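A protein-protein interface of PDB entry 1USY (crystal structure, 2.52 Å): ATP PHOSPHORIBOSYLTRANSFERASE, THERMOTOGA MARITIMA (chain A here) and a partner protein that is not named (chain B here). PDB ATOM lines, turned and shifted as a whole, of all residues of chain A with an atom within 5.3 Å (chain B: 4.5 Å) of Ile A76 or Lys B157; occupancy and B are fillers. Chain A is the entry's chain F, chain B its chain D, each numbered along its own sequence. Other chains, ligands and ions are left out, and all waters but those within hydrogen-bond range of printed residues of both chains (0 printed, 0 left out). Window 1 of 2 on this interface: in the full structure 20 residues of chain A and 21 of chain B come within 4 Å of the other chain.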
ATOM      1  N   SER A  74      -1.527 -30.146  -9.657  1.00  0.00           N
ATOM      2  CA  SER A  74      -1.590 -30.699  -8.331  1.00  0.00           C
ATOM      3  C   SER A  74      -0.179 -30.964  -7.749  1.00  0.00           C
ATOM      4  O   SER A  74       0.114 -32.076  -7.299  1.00  0.00           O
ATOM      5  CB  SER A  74      -2.327 -32.059  -8.452  1.00  0.00           C
ATOM      6  OG  SER A  74      -2.695 -32.383  -9.802  1.00  0.00           O
ATOM      7  N   LEU A  75       0.718 -29.998  -7.731  1.00  0.00           N
ATOM      8  CA  LEU A  75       2.073 -30.417  -7.419  1.00  0.00           C
ATOM      9  C   LEU A  75       2.584 -30.027  -6.024  1.00  0.00           C
ATOM     10  O   LEU A  75       1.837 -30.011  -5.043  1.00  0.00           O
ATOM     11  CB  LEU A  75       3.049 -29.951  -8.511  1.00  0.00           C
ATOM     12  CG  LEU A  75       2.564 -30.021  -9.965  1.00  0.00           C
ATOM     13  CD1 LEU A  75       3.069 -28.826 -10.768  1.00  0.00           C
ATOM     14  CD2 LEU A  75       2.988 -31.308 -10.611  1.00  0.00           C
ATOM     15  N   ILE A  76       3.877 -29.748  -5.949  1.00  0.00           N
ATOM     16  CA  ILE A  76       4.487 -29.262  -4.750  1.00  0.00           C
ATOM     17  C   ILE A  76       4.948 -27.867  -5.049  1.00  0.00           C
ATOM     18  O   ILE A  76       5.609 -27.622  -6.065  1.00  0.00           O
ATOM     19  CB  ILE A  76       5.633 -30.186  -4.296  1.00  0.00           C
ATOM     20  CG1 ILE A  76       5.022 -31.478  -3.732  1.00  0.00           C
ATOM     21  CG2 ILE A  76       6.452 -29.524  -3.194  1.00  0.00           C
ATOM     22  CD1 ILE A  76       6.002 -32.412  -3.101  1.00  0.00           C
ATOM     23  N   GLN A  77       4.557 -26.937  -4.189  1.00  0.00           N
ATOM     24  CA  GLN A  77       4.856 -25.534  -4.434  1.00  0.00           C
ATOM     25  C   GLN A  77       5.371 -24.953  -3.136  1.00  0.00           C
ATOM     26  O   GLN A  77       4.593 -24.369  -2.388  1.00  0.00           O
ATOM     27  CB  GLN A  77       3.632 -24.769  -4.955  1.00  0.00           C
ATOM     28  CG  GLN A  77       2.379 -25.578  -4.925  1.00  0.00           C
ATOM     29  CD  GLN A  77       1.186 -24.967  -5.649  1.00  0.00           C
ATOM     30  OE1 GLN A  77       1.008 -23.760  -5.637  1.00  0.00           O
ATOM     31  NE2 GLN A  77       0.336 -25.814  -6.210  1.00  0.00           N
ATOM     32  N   PRO A  78       6.678 -25.136  -2.876  1.00  0.00           N
ATOM     33  CA  PRO A  78       7.283 -24.797  -1.576  1.00  0.00           C
ATOM     34  C   PRO A  78       7.350 -23.317  -1.242  1.00  0.00           C
ATOM     35  O   PRO A  78       7.055 -23.005  -0.079  1.00  0.00           O
ATOM     36  CB  PRO A  78       8.702 -25.382  -1.650  1.00  0.00           C
ATOM     37  CG  PRO A  78       8.935 -25.776  -3.006  1.00  0.00           C
ATOM     38  CD  PRO A  78       7.656 -25.723  -3.806  1.00  0.00           C
ATOM     39  N   VAL A 173       7.540 -21.634  -7.306  1.00  0.00           N
ATOM     40  CA  VAL A 173       8.476 -22.652  -7.800  1.00  0.00           C
ATOM     41  C   VAL A 173       7.719 -23.923  -7.554  1.00  0.00           C
ATOM     42  O   VAL A 173       7.054 -24.036  -6.522  1.00  0.00           O
ATOM     43  CB  VAL A 173       9.824 -22.654  -7.055  1.00  0.00           C
ATOM     44  CG1 VAL A 173       9.629 -22.402  -5.615  1.00  0.00           C
ATOM     45  CG2 VAL A 173      10.532 -23.979  -7.211  1.00  0.00           C
ATOM     46  N   VAL A 174       7.732 -24.844  -8.509  1.00  0.00           N
ATOM     47  CA  VAL A 174       6.888 -26.029  -8.394  1.00  0.00           C
ATOM     48  C   VAL A 174       7.751 -27.266  -8.573  1.00  0.00           C
ATOM     49  O   VAL A 174       8.754 -27.224  -9.262  1.00  0.00           O
ATOM     50  CB  VAL A 174       5.727 -25.994  -9.415  1.00  0.00           C
ATOM     51  CG1 VAL A 174       4.741 -24.868  -9.106  1.00  0.00           C
ATOM     52  CG2 VAL A 174       6.255 -25.766 -10.778  1.00  0.00           C
ATOM     53  N   VAL A 175       7.386 -28.367  -7.937  1.00  0.00           N
ATOM     54  CA  VAL A 175       8.210 -29.581  -7.975  1.00  0.00           C
ATOM     55  C   VAL A 175       7.321 -30.796  -8.286  1.00  0.00           C
ATOM     56  O   VAL A 175       6.269 -30.996  -7.675  1.00  0.00           O
ATOM     57  CB  VAL A 175       8.932 -29.775  -6.610  1.00  0.00           C
ATOM     58  CG1 VAL A 175       9.807 -31.047  -6.554  1.00  0.00           C
ATOM     59  CG2 VAL A 175       9.748 -28.560  -6.287  1.00  0.00           C
ATOM     60  N   PRO A 177       6.137 -34.252  -7.718  1.00  0.00           N
ATOM     61  CA  PRO A 177       6.206 -34.910  -6.412  1.00  0.00           C
ATOM     62  C   PRO A 177       6.986 -36.210  -6.406  1.00  0.00           C
ATOM     63  O   PRO A 177       7.398 -36.623  -5.329  1.00  0.00           O
ATOM     64  CB  PRO A 177       4.743 -35.174  -6.035  1.00  0.00           C
ATOM     65  CG  PRO A 177       3.908 -34.673  -7.135  1.00  0.00           C
ATOM     66  CD  PRO A 177       4.791 -34.279  -8.301  1.00  0.00           C
ATOM     67  N   TYR A 180      10.844 -35.103  -6.213  1.00  0.00           N
ATOM     68  CA  TYR A 180      11.045 -34.687  -4.823  1.00  0.00           C
ATOM     69  C   TYR A 180      11.371 -35.871  -3.910  1.00  0.00           C
ATOM     70  O   TYR A 180      11.812 -35.713  -2.774  1.00  0.00           O
ATOM     71  CB  TYR A 180       9.782 -34.044  -4.277  1.00  0.00           C
ATOM     72  CG  TYR A 180      10.098 -33.008  -3.256  1.00  0.00           C
ATOM     73  CD1 TYR A 180      10.289 -33.346  -1.922  1.00  0.00           C
ATOM     74  CD2 TYR A 180      10.228 -31.686  -3.630  1.00  0.00           C
ATOM     75  CE1 TYR A 180      10.617 -32.385  -0.991  1.00  0.00           C
ATOM     76  CE2 TYR A 180      10.539 -30.715  -2.717  1.00  0.00           C
ATOM     77  CZ  TYR A 180      10.744 -31.057  -1.405  1.00  0.00           C
ATOM     78  OH  TYR A 180      11.052 -30.041  -0.526  1.00  0.00           O
ATOM     79  N   ARG A 181      11.117 -37.076  -4.362  1.00  0.00           N
ATOM     80  CA  ARG A 181      11.461 -38.172  -3.476  1.00  0.00           C
ATOM     81  C   ARG A 181      12.555 -39.032  -4.052  1.00  0.00           C
ATOM     82  O   ARG A 181      13.382 -39.546  -3.305  1.00  0.00           O
ATOM     83  CB  ARG A 181      10.205 -38.938  -3.049  1.00  0.00           C
ATOM     84  CG  ARG A 181       9.166 -37.929  -2.621  1.00  0.00           C
ATOM     85  CD  ARG A 181       7.797 -38.401  -2.667  1.00  0.00           C
ATOM     86  NE  ARG A 181       6.976 -37.913  -1.573  1.00  0.00           N
ATOM     87  CZ  ARG A 181       6.018 -36.993  -1.713  1.00  0.00           C
ATOM     88  NH1 ARG A 181       5.788 -36.398  -2.877  1.00  0.00           N
ATOM     89  NH2 ARG A 181       5.277 -36.655  -0.675  1.00  0.00           N
ATOM     90  N   LEU B 153      -2.678 -26.348   1.478  1.00  0.00           N
ATOM     91  CA  LEU B 153      -1.286 -25.952   1.603  1.00  0.00           C
ATOM     92  C   LEU B 153      -0.357 -27.058   2.132  1.00  0.00           C
ATOM     93  O   LEU B 153       0.808 -27.142   1.743  1.00  0.00           O
ATOM     94  CB  LEU B 153      -1.154 -24.611   2.325  1.00  0.00           C
ATOM     95  CG  LEU B 153      -1.248 -23.447   1.306  1.00  0.00           C
ATOM     96  CD1 LEU B 153      -2.519 -23.503   0.476  1.00  0.00           C
ATOM     97  CD2 LEU B 153      -1.212 -22.131   2.009  1.00  0.00           C
ATOM     98  N   ILE B 154      -0.906 -27.943   2.955  1.00  0.00           N
ATOM     99  CA  ILE B 154      -0.159 -29.070   3.475  1.00  0.00           C
ATOM    100  C   ILE B 154       0.138 -30.097   2.365  1.00  0.00           C
ATOM    101  O   ILE B 154       1.258 -30.612   2.243  1.00  0.00           O
ATOM    102  CB  ILE B 154      -0.933 -29.699   4.658  1.00  0.00           C
ATOM    103  CG1 ILE B 154      -0.331 -29.272   5.989  1.00  0.00           C
ATOM    104  CG2 ILE B 154      -0.916 -31.237   4.596  1.00  0.00           C
ATOM    105  CD1 ILE B 154      -1.374 -29.206   7.073  1.00  0.00           C
ATOM    106  N   ASP B 155      -0.888 -30.375   1.562  1.00  0.00           N
ATOM    107  CA  ASP B 155      -0.793 -31.263   0.420  1.00  0.00           C
ATOM    108  C   ASP B 155       0.217 -30.794  -0.611  1.00  0.00           C
ATOM    109  O   ASP B 155       0.912 -31.617  -1.214  1.00  0.00           O
ATOM    110  CB  ASP B 155      -2.160 -31.423  -0.247  1.00  0.00           C
ATOM    111  CG  ASP B 155      -2.151 -32.465  -1.351  1.00  0.00           C
ATOM    112  OD1 ASP B 155      -2.921 -32.316  -2.322  1.00  0.00           O
ATOM    113  OD2 ASP B 155      -1.395 -33.474  -1.362  1.00  0.00           O
ATOM    114  N   THR B 156       0.285 -29.479  -0.800  1.00  0.00           N
ATOM    115  CA  THR B 156       1.211 -28.857  -1.728  1.00  0.00           C
ATOM    116  C   THR B 156       2.573 -28.526  -1.140  1.00  0.00           C
ATOM    117  O   THR B 156       3.472 -28.047  -1.880  1.00  0.00           O
ATOM    118  CB  THR B 156       0.621 -27.542  -2.334  1.00  0.00           C
ATOM    119  OG1 THR B 156      -0.360 -26.968  -1.456  1.00  0.00           O
ATOM    120  CG2 THR B 156      -0.166 -27.865  -3.570  1.00  0.00           C
ATOM    121  N   LYS B 157       2.710 -28.720   0.174  1.00  0.00           N
ATOM    122  CA  LYS B 157       3.946 -28.402   0.920  1.00  0.00           C
ATOM    123  C   LYS B 157       4.330 -26.915   0.884  1.00  0.00           C
ATOM    124  O   LYS B 157       5.518 -26.550   0.937  1.00  0.00           O
ATOM    125  CB  LYS B 157       5.103 -29.271   0.427  1.00  0.00           C
ATOM    126  CG  LYS B 157       5.091 -30.708   0.939  1.00  0.00           C
ATOM    127  CD  LYS B 157       6.325 -31.405   0.419  1.00  0.00           C
ATOM    128  CE  LYS B 157       6.660 -32.698   1.151  1.00  0.00           C
ATOM    129  NZ  LYS B 157       5.873 -33.760   0.557  1.00  0.00           N
ATOM    130  N   ASN B 158       3.307 -26.064   0.790  1.00  0.00           N
ATOM    131  CA  ASN B 158       3.473 -24.623   0.656  1.00  0.00           C
ATOM    132  C   ASN B 158       3.687 -24.007   2.013  1.00  0.00           C
ATOM    133  O   ASN B 158       2.814 -23.283   2.533  1.00  0.00           O
ATOM    134  CB  ASN B 158       2.251 -24.010   0.003  1.00  0.00           C
ATOM    135  CG  ASN B 158       2.492 -22.599  -0.510  1.00  0.00           C
ATOM    136  OD1 ASN B 158       3.518 -21.966  -0.215  1.00  0.00           O
ATOM    137  ND2 ASN B 158       1.540 -22.093  -1.284  1.00  0.00           N
ATOM    138  N   LEU B 159       4.848 -24.319   2.588  1.00  0.00           N
ATOM    139  CA  LEU B 159       5.314 -23.701   3.833  1.00  0.00           C
ATOM    140  C   LEU B 159       5.188 -22.180   3.784  1.00  0.00           C
ATOM    141  O   LEU B 159       4.688 -21.549   4.734  1.00  0.00           O
ATOM    142  CB  LEU B 159       6.775 -24.054   4.065  1.00  0.00           C
ATOM    143  CG  LEU B 159       7.094 -24.701   5.403  1.00  0.00           C
ATOM    144  CD1 LEU B 159       8.580 -24.576   5.689  1.00  0.00           C
ATOM    145  CD2 LEU B 159       6.292 -24.066   6.528  1.00  0.00           C
ATOM    146  N   ILE B 180       5.244 -30.207   7.652  1.00  0.00           N
ATOM    147  CA  ILE B 180       5.778 -29.926   6.339  1.00  0.00           C
ATOM    148  C   ILE B 180       7.278 -30.004   6.390  1.00  0.00           C
ATOM    149  O   ILE B 180       7.901 -30.686   5.569  1.00  0.00           O
ATOM    150  CB  ILE B 180       5.316 -28.561   5.797  1.00  0.00           C
ATOM    151  CG1 ILE B 180       3.809 -28.592   5.579  1.00  0.00           C
ATOM    152  CG2 ILE B 180       6.060 -28.255   4.494  1.00  0.00           C
ATOM    153  CD1 ILE B 180       3.225 -27.324   4.984  1.00  0.00           C
ATOM    154  N   SER B 183       8.622 -33.474   6.692  1.00  0.00           N
ATOM    155  CA  SER B 183       8.444 -34.230   5.446  1.00  0.00           C
ATOM    156  C   SER B 183       9.587 -33.978   4.460  1.00  0.00           C
ATOM    157  O   SER B 183       9.695 -34.651   3.449  1.00  0.00           O
ATOM    158  CB  SER B 183       7.138 -33.845   4.789  1.00  0.00           C
ATOM    159  OG  SER B 183       7.297 -32.565   4.204  1.00  0.00           O
ATOM    160  N   ASP B 224       6.019 -39.314   5.959  1.00  0.00           N
ATOM    161  CA  ASP B 224       5.568 -38.062   5.348  1.00  0.00           C
ATOM    162  C   ASP B 224       4.084 -37.895   5.626  1.00  0.00           C
ATOM    163  O   ASP B 224       3.267 -38.590   5.032  1.00  0.00           O
ATOM    164  CB  ASP B 224       5.853 -38.080   3.843  1.00  0.00           C
ATOM    165  CG  ASP B 224       5.524 -36.776   3.141  1.00  0.00           C
ATOM    166  OD1 ASP B 224       4.582 -36.061   3.572  1.00  0.00           O
ATOM    167  OD2 ASP B 224       6.153 -36.398   2.102  1.00  0.00           O
ATOM    168  N   THR B 226       2.135 -35.288   4.947  1.00  0.00           N
ATOM    169  CA  THR B 226       1.532 -34.173   4.187  1.00  0.00           C
ATOM    170  C   THR B 226       0.474 -34.567   3.164  1.00  0.00           C
ATOM    171  O   THR B 226      -0.187 -33.698   2.603  1.00  0.00           O
ATOM    172  CB  THR B 226       2.609 -33.305   3.476  1.00  0.00           C
ATOM    173  OG1 THR B 226       3.314 -34.098   2.493  1.00  0.00           O
ATOM    174  CG2 THR B 226       3.670 -32.825   4.507  1.00  0.00           C
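Ser A74 touches none of the printed residues of chain B.
Of the printed residues of chain B, Leu A75 touches Thr B156.
Val A173 touches none of the printed residues of chain B.
Printed residues of chain A within 4 Å of Thr B156: Leu A75 (3.3 Å), Ile A76 (3.3 Å) and Gln A77 (2.8 Å).
Lys B157 touches just these residues of chain A: Ile A76, Pro A78 and Arg A181.
Of the printed residues of chain A, Asn B158 touches Gln A77 (3.3 Å) and Pro A78 (3.7 Å).
Printed residues of chain A within 4 Å of Leu B159: Pro A78.
The side-chain carboxylate (OD2) of Asp B224 lies within salt-bridge range of the side-chain amino group (NZ) of Lys B157, 3.1 Å away.
The backbone carbonyl oxygen (O) of Ile A76 lies within hydrogen-bond range of the backbone NH (N) of Val A175 (2.7 Å).
The guanidinium group (NH1) of Arg A181 is in hydrogen-bond range of the backbone carbonyl oxygen (O) of Pro A177 (2.9 Å).
The backbone carbonyl oxygen (O) of Leu B153 is in hydrogen-bond range of the backbone NH (N) of Asn B158 (2.9 Å).
The side-chain amino group (NZ) of Lys B157 lies within hydrogen-bond range of the side-chain hydroxyl (OG1) of Thr B226 (3.2 Å).
The backbone carbonyl oxygen (O) of Leu B153 sits close to the side-chain hydroxyl (OG1) of Thr B156 (3.4 Å).
Of the 11 printed residues of chain A, 5 touch a printed residue of chain B.
Hydrophobic or aromatic side chains of chain A within 4 Å of the printed part of chain B: Ile A76.
Along chain A the printed residues that touch a printed residue of chain B span positions 75 to 181.
Among the printed residues, Asp or Glu carboxylates within 4 Å of a Lys or Arg side-chain nitrogen of the other chain: Arg A181 with Asp B224.
Thr B156 touches Leu A75 (CG2 to O, 3.3 Å).
O of Thr B156 touches CA of Ile A76 (3.3 Å).
Lys B157 touches Ile A76 (CD to CD1, 3.7 Å).
CA of Pro A78 touches O of Lys B157, 3.5 Å away.
Asn B158 touches Pro A78 (OD1 to O, 3.7 Å).
O of Pro A78 touches N of Leu B159 (3.7 Å).
The backbone carbonyl oxygen (O) of Gln A77 lies close to the side-chain amide oxygen (OD1) of Asn B158, at 3.4 Å.
The side-chain amino group (NZ) of Lys B157 sits close to the guanidinium group (NH2) of Arg A181 (3.2 Å).
The side-chain carboxylate of Asp B224 is in salt-bridge range of the guanidinium group of Arg A181, at 2.9 Å.
The backbone carbonyl oxygen (O) of Thr B156 sits at hydrogen-bond distance from the backbone NH (N) of Gln A77, 2.8 Å away.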
